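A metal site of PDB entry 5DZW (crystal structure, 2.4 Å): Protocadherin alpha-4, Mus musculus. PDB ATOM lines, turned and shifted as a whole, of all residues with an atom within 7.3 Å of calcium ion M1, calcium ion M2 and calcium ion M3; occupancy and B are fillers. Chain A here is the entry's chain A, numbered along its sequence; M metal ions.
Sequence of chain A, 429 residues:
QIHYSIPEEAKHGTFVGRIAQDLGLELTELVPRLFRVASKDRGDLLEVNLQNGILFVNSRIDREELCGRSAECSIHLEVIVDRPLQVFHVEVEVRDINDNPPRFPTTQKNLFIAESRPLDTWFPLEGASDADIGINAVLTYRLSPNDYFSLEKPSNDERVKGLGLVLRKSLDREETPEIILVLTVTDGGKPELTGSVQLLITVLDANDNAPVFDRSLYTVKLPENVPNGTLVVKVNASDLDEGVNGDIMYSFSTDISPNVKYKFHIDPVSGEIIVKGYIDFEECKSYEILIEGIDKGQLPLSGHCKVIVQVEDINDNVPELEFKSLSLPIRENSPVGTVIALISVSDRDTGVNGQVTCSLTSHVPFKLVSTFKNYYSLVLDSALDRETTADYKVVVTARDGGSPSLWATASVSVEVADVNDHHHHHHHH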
ATOM      1  N   GLU A 115      10.703 -19.565  -5.363  1.00  0.00           N
ATOM      2  CA  GLU A 115       9.931 -18.341  -5.143  1.00  0.00           C
ATOM      3  C   GLU A 115       9.267 -17.875  -6.442  1.00  0.00           C
ATOM      4  O   GLU A 115       8.295 -17.121  -6.415  1.00  0.00           O
ATOM      5  CB  GLU A 115      10.845 -17.245  -4.595  1.00  0.00           C
ATOM      6  CG  GLU A 115      10.140 -15.961  -4.194  1.00  0.00           C
ATOM      7  CD  GLU A 115      11.102 -14.833  -3.903  1.00  0.00           C
ATOM      8  OE1 GLU A 115      12.329 -15.062  -3.953  1.00  0.00           O
ATOM      9  OE2 GLU A 115      10.634 -13.705  -3.634  1.00  0.00           O
ATOM     10  N   LEU A 171       4.393 -16.083  -2.985  1.00  0.00           N
ATOM     11  CA  LEU A 171       5.410 -16.425  -1.992  1.00  0.00           C
ATOM     12  C   LEU A 171       6.650 -15.548  -2.145  1.00  0.00           C
ATOM     13  O   LEU A 171       7.093 -15.266  -3.258  1.00  0.00           O
ATOM     14  CB  LEU A 171       5.785 -17.906  -2.105  1.00  0.00           C
ATOM     15  CG  LEU A 171       6.632 -18.410  -3.277  1.00  0.00           C
ATOM     16  CD1 LEU A 171       7.102 -19.830  -3.010  1.00  0.00           C
ATOM     17  CD2 LEU A 171       5.877 -18.349  -4.608  1.00  0.00           C
ATOM     18  N   ASP A 172       7.207 -15.123  -1.019  1.00  0.00           N
ATOM     19  CA  ASP A 172       8.380 -14.267  -1.013  1.00  0.00           C
ATOM     20  C   ASP A 172       9.434 -14.772  -0.023  1.00  0.00           C
ATOM     21  O   ASP A 172       9.183 -14.830   1.176  1.00  0.00           O
ATOM     22  CB  ASP A 172       7.991 -12.823  -0.681  1.00  0.00           C
ATOM     23  CG  ASP A 172       9.184 -11.878  -0.687  1.00  0.00           C
ATOM     24  OD1 ASP A 172       9.556 -11.411  -1.788  1.00  0.00           O
ATOM     25  OD2 ASP A 172       9.739 -11.604   0.393  1.00  0.00           O
ATOM     26  N   ARG A 173      10.602 -15.112  -0.545  1.00  0.00           N
ATOM     27  CA  ARG A 173      11.694 -15.651   0.250  1.00  0.00           C
ATOM     28  C   ARG A 173      12.162 -14.675   1.341  1.00  0.00           C
ATOM     29  O   ARG A 173      12.459 -15.094   2.461  1.00  0.00           O
ATOM     30  CB  ARG A 173      12.858 -16.042  -0.654  1.00  0.00           C
ATOM     31  CG  ARG A 173      14.170 -16.314   0.056  1.00  0.00           C
ATOM     32  CD  ARG A 173      15.176 -15.199  -0.209  1.00  0.00           C
ATOM     33  NE  ARG A 173      16.516 -15.549   0.246  1.00  0.00           N
ATOM     34  CZ  ARG A 173      16.986 -15.269   1.459  1.00  0.00           C
ATOM     35  NH1 ARG A 173      18.220 -15.618   1.794  1.00  0.00           N
ATOM     36  NH2 ARG A 173      16.221 -14.640   2.337  1.00  0.00           N
ATOM     37  N   GLU A 174      12.225 -13.397   1.006  1.00  0.00           N
ATOM     38  CA  GLU A 174      12.710 -12.383   1.930  1.00  0.00           C
ATOM     39  C   GLU A 174      11.770 -12.164   3.114  1.00  0.00           C
ATOM     40  O   GLU A 174      12.209 -11.932   4.231  1.00  0.00           O
ATOM     41  CB  GLU A 174      12.948 -11.051   1.205  1.00  0.00           C
ATOM     42  CG  GLU A 174      14.188 -11.020   0.328  1.00  0.00           C
ATOM     43  CD  GLU A 174      14.048 -11.857  -0.929  1.00  0.00           C
ATOM     44  OE1 GLU A 174      12.901 -12.148  -1.325  1.00  0.00           O
ATOM     45  OE2 GLU A 174      15.090 -12.229  -1.515  1.00  0.00           O
ATOM     46  N   GLU A 175      10.469 -12.244   2.843  1.00  0.00           N
ATOM     47  CA  GLU A 175       9.471 -12.065   3.896  1.00  0.00           C
ATOM     48  C   GLU A 175       9.449 -13.260   4.851  1.00  0.00           C
ATOM     49  O   GLU A 175       9.591 -13.097   6.067  1.00  0.00           O
ATOM     50  CB  GLU A 175       8.083 -11.856   3.284  1.00  0.00           C
ATOM     51  CG  GLU A 175       6.973 -11.659   4.303  1.00  0.00           C
ATOM     52  CD  GLU A 175       5.646 -11.303   3.671  1.00  0.00           C
ATOM     53  OE1 GLU A 175       5.660 -10.752   2.544  1.00  0.00           O
ATOM     54  OE2 GLU A 175       4.594 -11.564   4.281  1.00  0.00           O
ATOM     55  N   LEU A 204      13.104 -21.069  -2.121  1.00  0.00           N
ATOM     56  CA  LEU A 204      14.376 -20.761  -2.751  1.00  0.00           C
ATOM     57  C   LEU A 204      14.440 -19.297  -3.183  1.00  0.00           C
ATOM     58  O   LEU A 204      13.421 -18.683  -3.489  1.00  0.00           O
ATOM     59  CB  LEU A 204      14.613 -21.686  -3.945  1.00  0.00           C
ATOM     60  CG  LEU A 204      14.459 -23.179  -3.656  1.00  0.00           C
ATOM     61  CD1 LEU A 204      14.657 -24.019  -4.911  1.00  0.00           C
ATOM     62  CD2 LEU A 204      15.412 -23.620  -2.548  1.00  0.00           C
ATOM     63  N   ASP A 205      15.651 -18.742  -3.195  1.00  0.00           N
ATOM     64  CA  ASP A 205      15.833 -17.325  -3.523  1.00  0.00           C
ATOM     65  C   ASP A 205      15.753 -17.069  -5.028  1.00  0.00           C
ATOM     66  O   ASP A 205      16.562 -17.591  -5.800  1.00  0.00           O
ATOM     67  CB  ASP A 205      17.170 -16.828  -2.980  1.00  0.00           C
ATOM     68  CG  ASP A 205      17.405 -15.354  -3.268  1.00  0.00           C
ATOM     69  OD1 ASP A 205      16.433 -14.578  -3.231  1.00  0.00           O
ATOM     70  OD2 ASP A 205      18.565 -14.975  -3.530  1.00  0.00           O
ATOM     71  N   ALA A 206      14.777 -16.273  -5.431  1.00  0.00           N
ATOM     72  CA  ALA A 206      14.639 -15.863  -6.825  1.00  0.00           C
ATOM     73  C   ALA A 206      15.222 -14.465  -7.012  1.00  0.00           C
ATOM     74  O   ALA A 206      15.303 -13.698  -6.062  1.00  0.00           O
ATOM     75  CB  ALA A 206      13.191 -15.910  -7.256  1.00  0.00           C
ATOM     76  N   ASN A 207      15.607 -14.147  -8.234  1.00  0.00           N
ATOM     77  CA  ASN A 207      16.159 -12.818  -8.529  1.00  0.00           C
ATOM     78  C   ASN A 207      15.049 -11.848  -8.936  1.00  0.00           C
ATOM     79  O   ASN A 207      14.963 -11.432 -10.085  1.00  0.00           O
ATOM     80  CB  ASN A 207      17.212 -12.904  -9.633  1.00  0.00           C
ATOM     81  CG  ASN A 207      18.004 -11.621  -9.770  1.00  0.00           C
ATOM     82  OD1 ASN A 207      18.141 -10.853  -8.823  1.00  0.00           O
ATOM     83  ND2 ASN A 207      18.522 -11.371 -10.975  1.00  0.00           N
ATOM     84  N   ASP A 208      14.200 -11.503  -7.975  1.00  0.00           N
ATOM     85  CA  ASP A 208      13.041 -10.666  -8.251  1.00  0.00           C
ATOM     86  C   ASP A 208      13.096  -9.328  -7.514  1.00  0.00           C
ATOM     87  O   ASP A 208      12.100  -8.606  -7.442  1.00  0.00           O
ATOM     88  CB  ASP A 208      11.749 -11.407  -7.887  1.00  0.00           C
ATOM     89  CG  ASP A 208      11.739 -11.890  -6.450  1.00  0.00           C
ATOM     90  OD1 ASP A 208      12.818 -12.249  -5.935  1.00  0.00           O
ATOM     91  OD2 ASP A 208      10.644 -11.912  -5.843  1.00  0.00           O
ATOM     92  N   ASN A 209      14.264  -8.993  -6.967  1.00  0.00           N
ATOM     93  CA  ASN A 209      14.453  -7.717  -6.304  1.00  0.00           C
ATOM     94  C   ASN A 209      15.647  -6.940  -6.850  1.00  0.00           C
ATOM     95  O   ASN A 209      16.765  -7.461  -6.904  1.00  0.00           O
ATOM     96  CB  ASN A 209      14.613  -7.906  -4.796  1.00  0.00           C
ATOM     97  CG  ASN A 209      13.280  -8.028  -4.074  1.00  0.00           C
ATOM     98  OD1 ASN A 209      12.320  -8.565  -4.624  1.00  0.00           O
ATOM     99  ND2 ASN A 209      13.224  -7.517  -2.852  1.00  0.00           N
ATOM    100  N   ALA A 210      15.400  -5.704  -7.268  1.00  0.00           N
ATOM    101  CA  ALA A 210      16.451  -4.844  -7.808  1.00  0.00           C
ATOM    102  C   ALA A 210      17.201  -4.137  -6.678  1.00  0.00           C
ATOM    103  O   ALA A 210      16.632  -3.866  -5.621  1.00  0.00           O
ATOM    104  CB  ALA A 210      15.847  -3.828  -8.765  1.00  0.00           C
ATOM    105  N   PRO A 211      18.495  -3.836  -6.902  1.00  0.00           N
ATOM    106  CA  PRO A 211      19.284  -3.099  -5.925  1.00  0.00           C
ATOM    107  C   PRO A 211      18.759  -1.686  -5.696  1.00  0.00           C
ATOM    108  O   PRO A 211      18.171  -1.099  -6.608  1.00  0.00           O
ATOM    109  CB  PRO A 211      20.683  -3.070  -6.552  1.00  0.00           C
ATOM    110  CG  PRO A 211      20.471  -3.326  -8.000  1.00  0.00           C
ATOM    111  CD  PRO A 211      19.290  -4.248  -8.069  1.00  0.00           C
ATOM    112  N   ASP A 239      20.647  -4.784  -1.693  1.00  0.00           N
ATOM    113  CA  ASP A 239      19.744  -5.680  -2.402  1.00  0.00           C
ATOM    114  C   ASP A 239      19.317  -6.840  -1.504  1.00  0.00           C
ATOM    115  O   ASP A 239      20.138  -7.426  -0.801  1.00  0.00           O
ATOM    116  CB  ASP A 239      20.406  -6.198  -3.684  1.00  0.00           C
ATOM    117  CG  ASP A 239      19.444  -6.955  -4.580  1.00  0.00           C
ATOM    118  OD1 ASP A 239      18.212  -6.853  -4.358  1.00  0.00           O
ATOM    119  OD2 ASP A 239      19.914  -7.640  -5.504  1.00  0.00           O
ATOM    120  N   LEU A 240      18.024  -7.166  -1.548  1.00  0.00           N
ATOM    121  CA  LEU A 240      17.455  -8.136  -0.622  1.00  0.00           C
ATOM    122  C   LEU A 240      17.768  -9.586  -0.987  1.00  0.00           C
ATOM    123  O   LEU A 240      17.731 -10.463  -0.131  1.00  0.00           O
ATOM    124  CB  LEU A 240      15.940  -7.940  -0.536  1.00  0.00           C
ATOM    125  CG  LEU A 240      15.489  -6.637   0.115  1.00  0.00           C
ATOM    126  CD1 LEU A 240      13.973  -6.578   0.227  1.00  0.00           C
ATOM    127  CD2 LEU A 240      16.131  -6.474   1.489  1.00  0.00           C
ATOM    128  N   ASP A 241      18.087  -9.832  -2.252  1.00  0.00           N
ATOM    129  CA  ASP A 241      18.417 -11.186  -2.690  1.00  0.00           C
ATOM    130  C   ASP A 241      19.794 -11.610  -2.195  1.00  0.00           C
ATOM    131  O   ASP A 241      20.587 -10.775  -1.750  1.00  0.00           O
ATOM    132  CB  ASP A 241      18.339 -11.294  -4.217  1.00  0.00           C
ATOM    133  CG  ASP A 241      16.964 -10.979  -4.756  1.00  0.00           C
ATOM    134  OD1 ASP A 241      16.040 -10.764  -3.946  1.00  0.00           O
ATOM    135  OD2 ASP A 241      16.796 -10.964  -5.991  1.00  0.00           O
ATOM    136  N   GLU A 242      20.073 -12.905  -2.270  1.00  0.00           N
ATOM    137  CA  GLU A 242      21.333 -13.446  -1.762  1.00  0.00           C
ATOM    138  C   GLU A 242      22.170 -14.082  -2.873  1.00  0.00           C
ATOM    139  O   GLU A 242      21.681 -14.307  -3.978  1.00  0.00           O
ATOM    140  CB  GLU A 242      21.062 -14.470  -0.660  1.00  0.00           C
ATOM    141  N   VAL A 244      24.854 -14.458  -5.841  1.00  0.00           N
ATOM    142  CA  VAL A 244      25.198 -13.610  -6.965  1.00  0.00           C
ATOM    143  C   VAL A 244      24.034 -12.680  -7.309  1.00  0.00           C
ATOM    144  O   VAL A 244      24.208 -11.672  -7.988  1.00  0.00           O
ATOM    145  CB  VAL A 244      25.581 -14.431  -8.211  1.00  0.00           C
ATOM    146  CG1 VAL A 244      26.846 -15.232  -7.959  1.00  0.00           C
ATOM    147  CG2 VAL A 244      24.436 -15.351  -8.627  1.00  0.00           C
ATOM    148  N   ASN A 245      22.838 -13.034  -6.833  1.00  0.00           N
ATOM    149  CA  ASN A 245      21.666 -12.200  -7.024  1.00  0.00           C
ATOM    150  C   ASN A 245      21.664 -11.020  -6.062  1.00  0.00           C
ATOM    151  O   ASN A 245      20.842 -10.115  -6.179  1.00  0.00           O
ATOM    152  CB  ASN A 245      20.387 -13.019  -6.850  1.00  0.00           C
ATOM    153  CG  ASN A 245      20.266 -14.137  -7.873  1.00  0.00           C
ATOM    154  OD1 ASN A 245      21.171 -14.355  -8.669  1.00  0.00           O
ATOM    155  ND2 ASN A 245      19.149 -14.841  -7.837  1.00  0.00           N
ATOM    156  N   GLY A 246      22.601 -11.039  -5.122  1.00  0.00           N
ATOM    157  CA  GLY A 246      22.713  -9.983  -4.129  1.00  0.00           C
ATOM    158  C   GLY A 246      23.897  -9.058  -4.359  1.00  0.00           C
ATOM    159  O   GLY A 246      23.850  -7.875  -4.024  1.00  0.00           O
ATOM    160  N   ASP A 247      24.977  -9.603  -4.929  1.00  0.00           N
ATOM    161  CA  ASP A 247      26.178  -8.814  -5.199  1.00  0.00           C
ATOM    162  C   ASP A 247      25.926  -7.771  -6.279  1.00  0.00           C
ATOM    163  O   ASP A 247      25.330  -8.071  -7.309  1.00  0.00           O
ATOM    164  CB  ASP A 247      27.337  -9.729  -5.603  1.00  0.00           C
ATOM    165  CG  ASP A 247      27.885 -10.533  -4.441  1.00  0.00           C
ATOM    166  OD1 ASP A 247      27.093 -10.925  -3.557  1.00  0.00           O
ATOM    167  OD2 ASP A 247      29.105 -10.777  -4.408  1.00  0.00           O
ATOM    168  N   ILE A 248      26.389  -6.541  -6.032  1.00  0.00           N
ATOM    169  CA  ILE A 248      26.110  -5.426  -6.929  1.00  0.00           C
ATOM    170  C   ILE A 248      27.371  -4.848  -7.568  1.00  0.00           C
ATOM    171  O   ILE A 248      28.355  -4.569  -6.887  1.00  0.00           O
ATOM    172  CB  ILE A 248      25.380  -4.295  -6.177  1.00  0.00           C
ATOM    173  CG1 ILE A 248      24.202  -4.851  -5.371  1.00  0.00           C
ATOM    174  CG2 ILE A 248      24.903  -3.219  -7.152  1.00  0.00           C
ATOM    175  CD1 ILE A 248      23.542  -3.833  -4.475  1.00  0.00           C
ATOM    176  N   ASP A 295      22.937  -6.144 -10.355  1.00  0.00           N
ATOM    177  CA  ASP A 295      23.301  -7.386  -9.677  1.00  0.00           C
ATOM    178  C   ASP A 295      23.891  -8.394 -10.649  1.00  0.00           C
ATOM    179  O   ASP A 295      23.997  -8.135 -11.848  1.00  0.00           O
ATOM    180  CB  ASP A 295      22.087  -7.987  -8.946  1.00  0.00           C
ATOM    181  CG  ASP A 295      20.831  -7.976  -9.791  1.00  0.00           C
ATOM    182  OD1 ASP A 295      20.932  -8.152 -11.023  1.00  0.00           O
ATOM    183  OD2 ASP A 295      19.733  -7.797  -9.228  1.00  0.00           O
ATOM    184  N   LYS A 296      24.284  -9.561 -10.140  1.00  0.00           N
ATOM    185  CA  LYS A 296      24.971 -10.563 -10.950  1.00  0.00           C
ATOM    186  C   LYS A 296      24.163 -11.845 -11.097  1.00  0.00           C
ATOM    187  O   LYS A 296      24.715 -12.942 -11.025  1.00  0.00           O
ATOM    188  CB  LYS A 296      26.344 -10.872 -10.338  1.00  0.00           C
ATOM    189  CG  LYS A 296      27.230  -9.657 -10.129  1.00  0.00           C
ATOM    190  CD  LYS A 296      28.544 -10.039  -9.464  1.00  0.00           C
ATOM    191  N   GLY A 297      22.858 -11.708 -11.309  1.00  0.00           N
ATOM    192  CA  GLY A 297      21.994 -12.854 -11.490  1.00  0.00           C
ATOM    193  C   GLY A 297      21.897 -13.270 -12.939  1.00  0.00           C
ATOM    194  O   GLY A 297      22.485 -12.634 -13.819  1.00  0.00           O
ATOM    195  N   LEU A 299      19.113 -13.245 -14.800  1.00  0.00           N
ATOM    196  CA  LEU A 299      18.415 -12.100 -15.361  1.00  0.00           C
ATOM    197  C   LEU A 299      18.676 -10.891 -14.481  1.00  0.00           C
ATOM    198  O   LEU A 299      17.990 -10.698 -13.470  1.00  0.00           O
ATOM    199  CB  LEU A 299      16.915 -12.368 -15.488  1.00  0.00           C
ATOM    200  CG  LEU A 299      16.092 -11.233 -16.092  1.00  0.00           C
ATOM    201  CD1 LEU A 299      16.653 -10.826 -17.445  1.00  0.00           C
ATOM    202  CD2 LEU A 299      14.629 -11.619 -16.200  1.00  0.00           C
ATOM    203  N   PRO A 300      19.676 -10.078 -14.846  1.00  0.00           N
ATOM    204  CA  PRO A 300      20.134  -8.943 -14.035  1.00  0.00           C
ATOM    205  C   PRO A 300      19.069  -7.881 -13.823  1.00  0.00           C
ATOM    206  O   PRO A 300      18.327  -7.548 -14.758  1.00  0.00           O
ATOM    207  CB  PRO A 300      21.301  -8.384 -14.848  1.00  0.00           C
ATOM    208  CG  PRO A 300      21.739  -9.503 -15.736  1.00  0.00           C
ATOM    209  CD  PRO A 300      20.484 -10.242 -16.070  1.00  0.00           C
ATOM    210  N   LEU A 301      18.997  -7.353 -12.608  1.00  0.00           N
ATOM    211  CA  LEU A 301      18.137  -6.211 -12.308  1.00  0.00           C
ATOM    212  C   LEU A 301      18.999  -4.992 -11.980  1.00  0.00           C
ATOM    213  O   LEU A 301      20.066  -5.118 -11.373  1.00  0.00           O
ATOM    214  CB  LEU A 301      17.203  -6.526 -11.141  1.00  0.00           C
ATOM    215  CG  LEU A 301      16.113  -7.565 -11.420  1.00  0.00           C
ATOM    216  CD1 LEU A 301      15.168  -7.685 -10.234  1.00  0.00           C
ATOM    217  CD2 LEU A 301      15.350  -7.211 -12.688  1.00  0.00           C
HETATM  218 CA    CA M   1      14.654 -12.999  -3.893  1.00  0.00          CA
HETATM  219 CA    CA M   2      12.024 -11.698  -3.551  1.00  0.00          CA
HETATM  220 CA    CA M   3      18.660  -9.004  -6.977  1.00  0.00          CA
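Within 4 Å of calcium ion M3: Asn 207, Asn 209, Asp 239, Asp 241, Asn 245 and Asp 295.
OD1 of Asp 295 sits at hydrogen-bond distance from N of Leu 301, at 2.6 Å.
The backbone carbonyl oxygen (O) of Leu 204 sits close to the backbone NH (N) of Glu 115, 3.4 Å away.
NE of Arg 173 sits close to OD1 of Asp 205 (3.6 Å).
The side-chain carboxylate of Glu 115 is in hydrogen-bond range of the backbone NH of Ala 206 (3.1 Å).
The backbone NH (N) of Glu 242 is in hydrogen-bond range of the side-chain carboxylate (OD2) of Asp 205.
O of Leu 299 sits at hydrogen-bond distance from ND2 of Asn 207, 2.6 Å away.
N of Glu 174 sits at hydrogen-bond distance from OD2 of Asp 172 (3.1 Å).
OE2 of Glu 115 lies close to N of Arg 173 (3.4 Å).
Calcium ion M1 is bound by the backbone carbonyl oxygen (O) of Ala 206 (2.4 Å), the side-chain carboxylate (OD1) of Asp 205 (2.5 Å), the side-chain carboxylate (OE2) of Glu 174 (2.5 Å), the side-chain carboxylate (OD1) of Asp 241 (2.6 Å) and the side-chain carboxylate (OD1) of Asp 208 (2.8 Å).
Slightly farther from calcium ion M1 lies OE1 of Glu 115 (3.1 Å).
Of the 29 residues printed, 5 come within 4 Å of calcium ion M2.
Calcium ion M2 is bound by OE1 of Glu 174, OE2 of Glu 115, OD1 of Asp 208 and OD2 of Asp 208.
Calcium ion M2 has four donor atoms within binding distance.
Slightly farther from calcium ion M2 lies OD1 of Asp 172 (3.0 Å).
Calcium ion M3 is bound by OD2 of Asp 239, at 2.4 Å.
The backbone carbonyl oxygen (O) of Asn 209 is bound to calcium ion M3.
O of Asn 245 binds calcium ion M3 (2.6 Å).
The side-chain amide oxygen (OD1) of Asn 207 binds calcium ion M3.
Calcium ion M3 is bound by the side-chain carboxylate (OD2) of Asp 295.
Calcium ion M3 is bound by the side-chain carboxylate (OD2) of Asp 241.
Calcium ion M3 has six donor atoms within binding distance.
Six residues have an atom within 4 Å of calcium ion M1: Glu 115, Glu 174, Asp 205, Ala 206, Asp 208 and Asp 241.
The nearest printed residue that does not touch calcium ion M1 is Arg 173 (4.3 Å).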
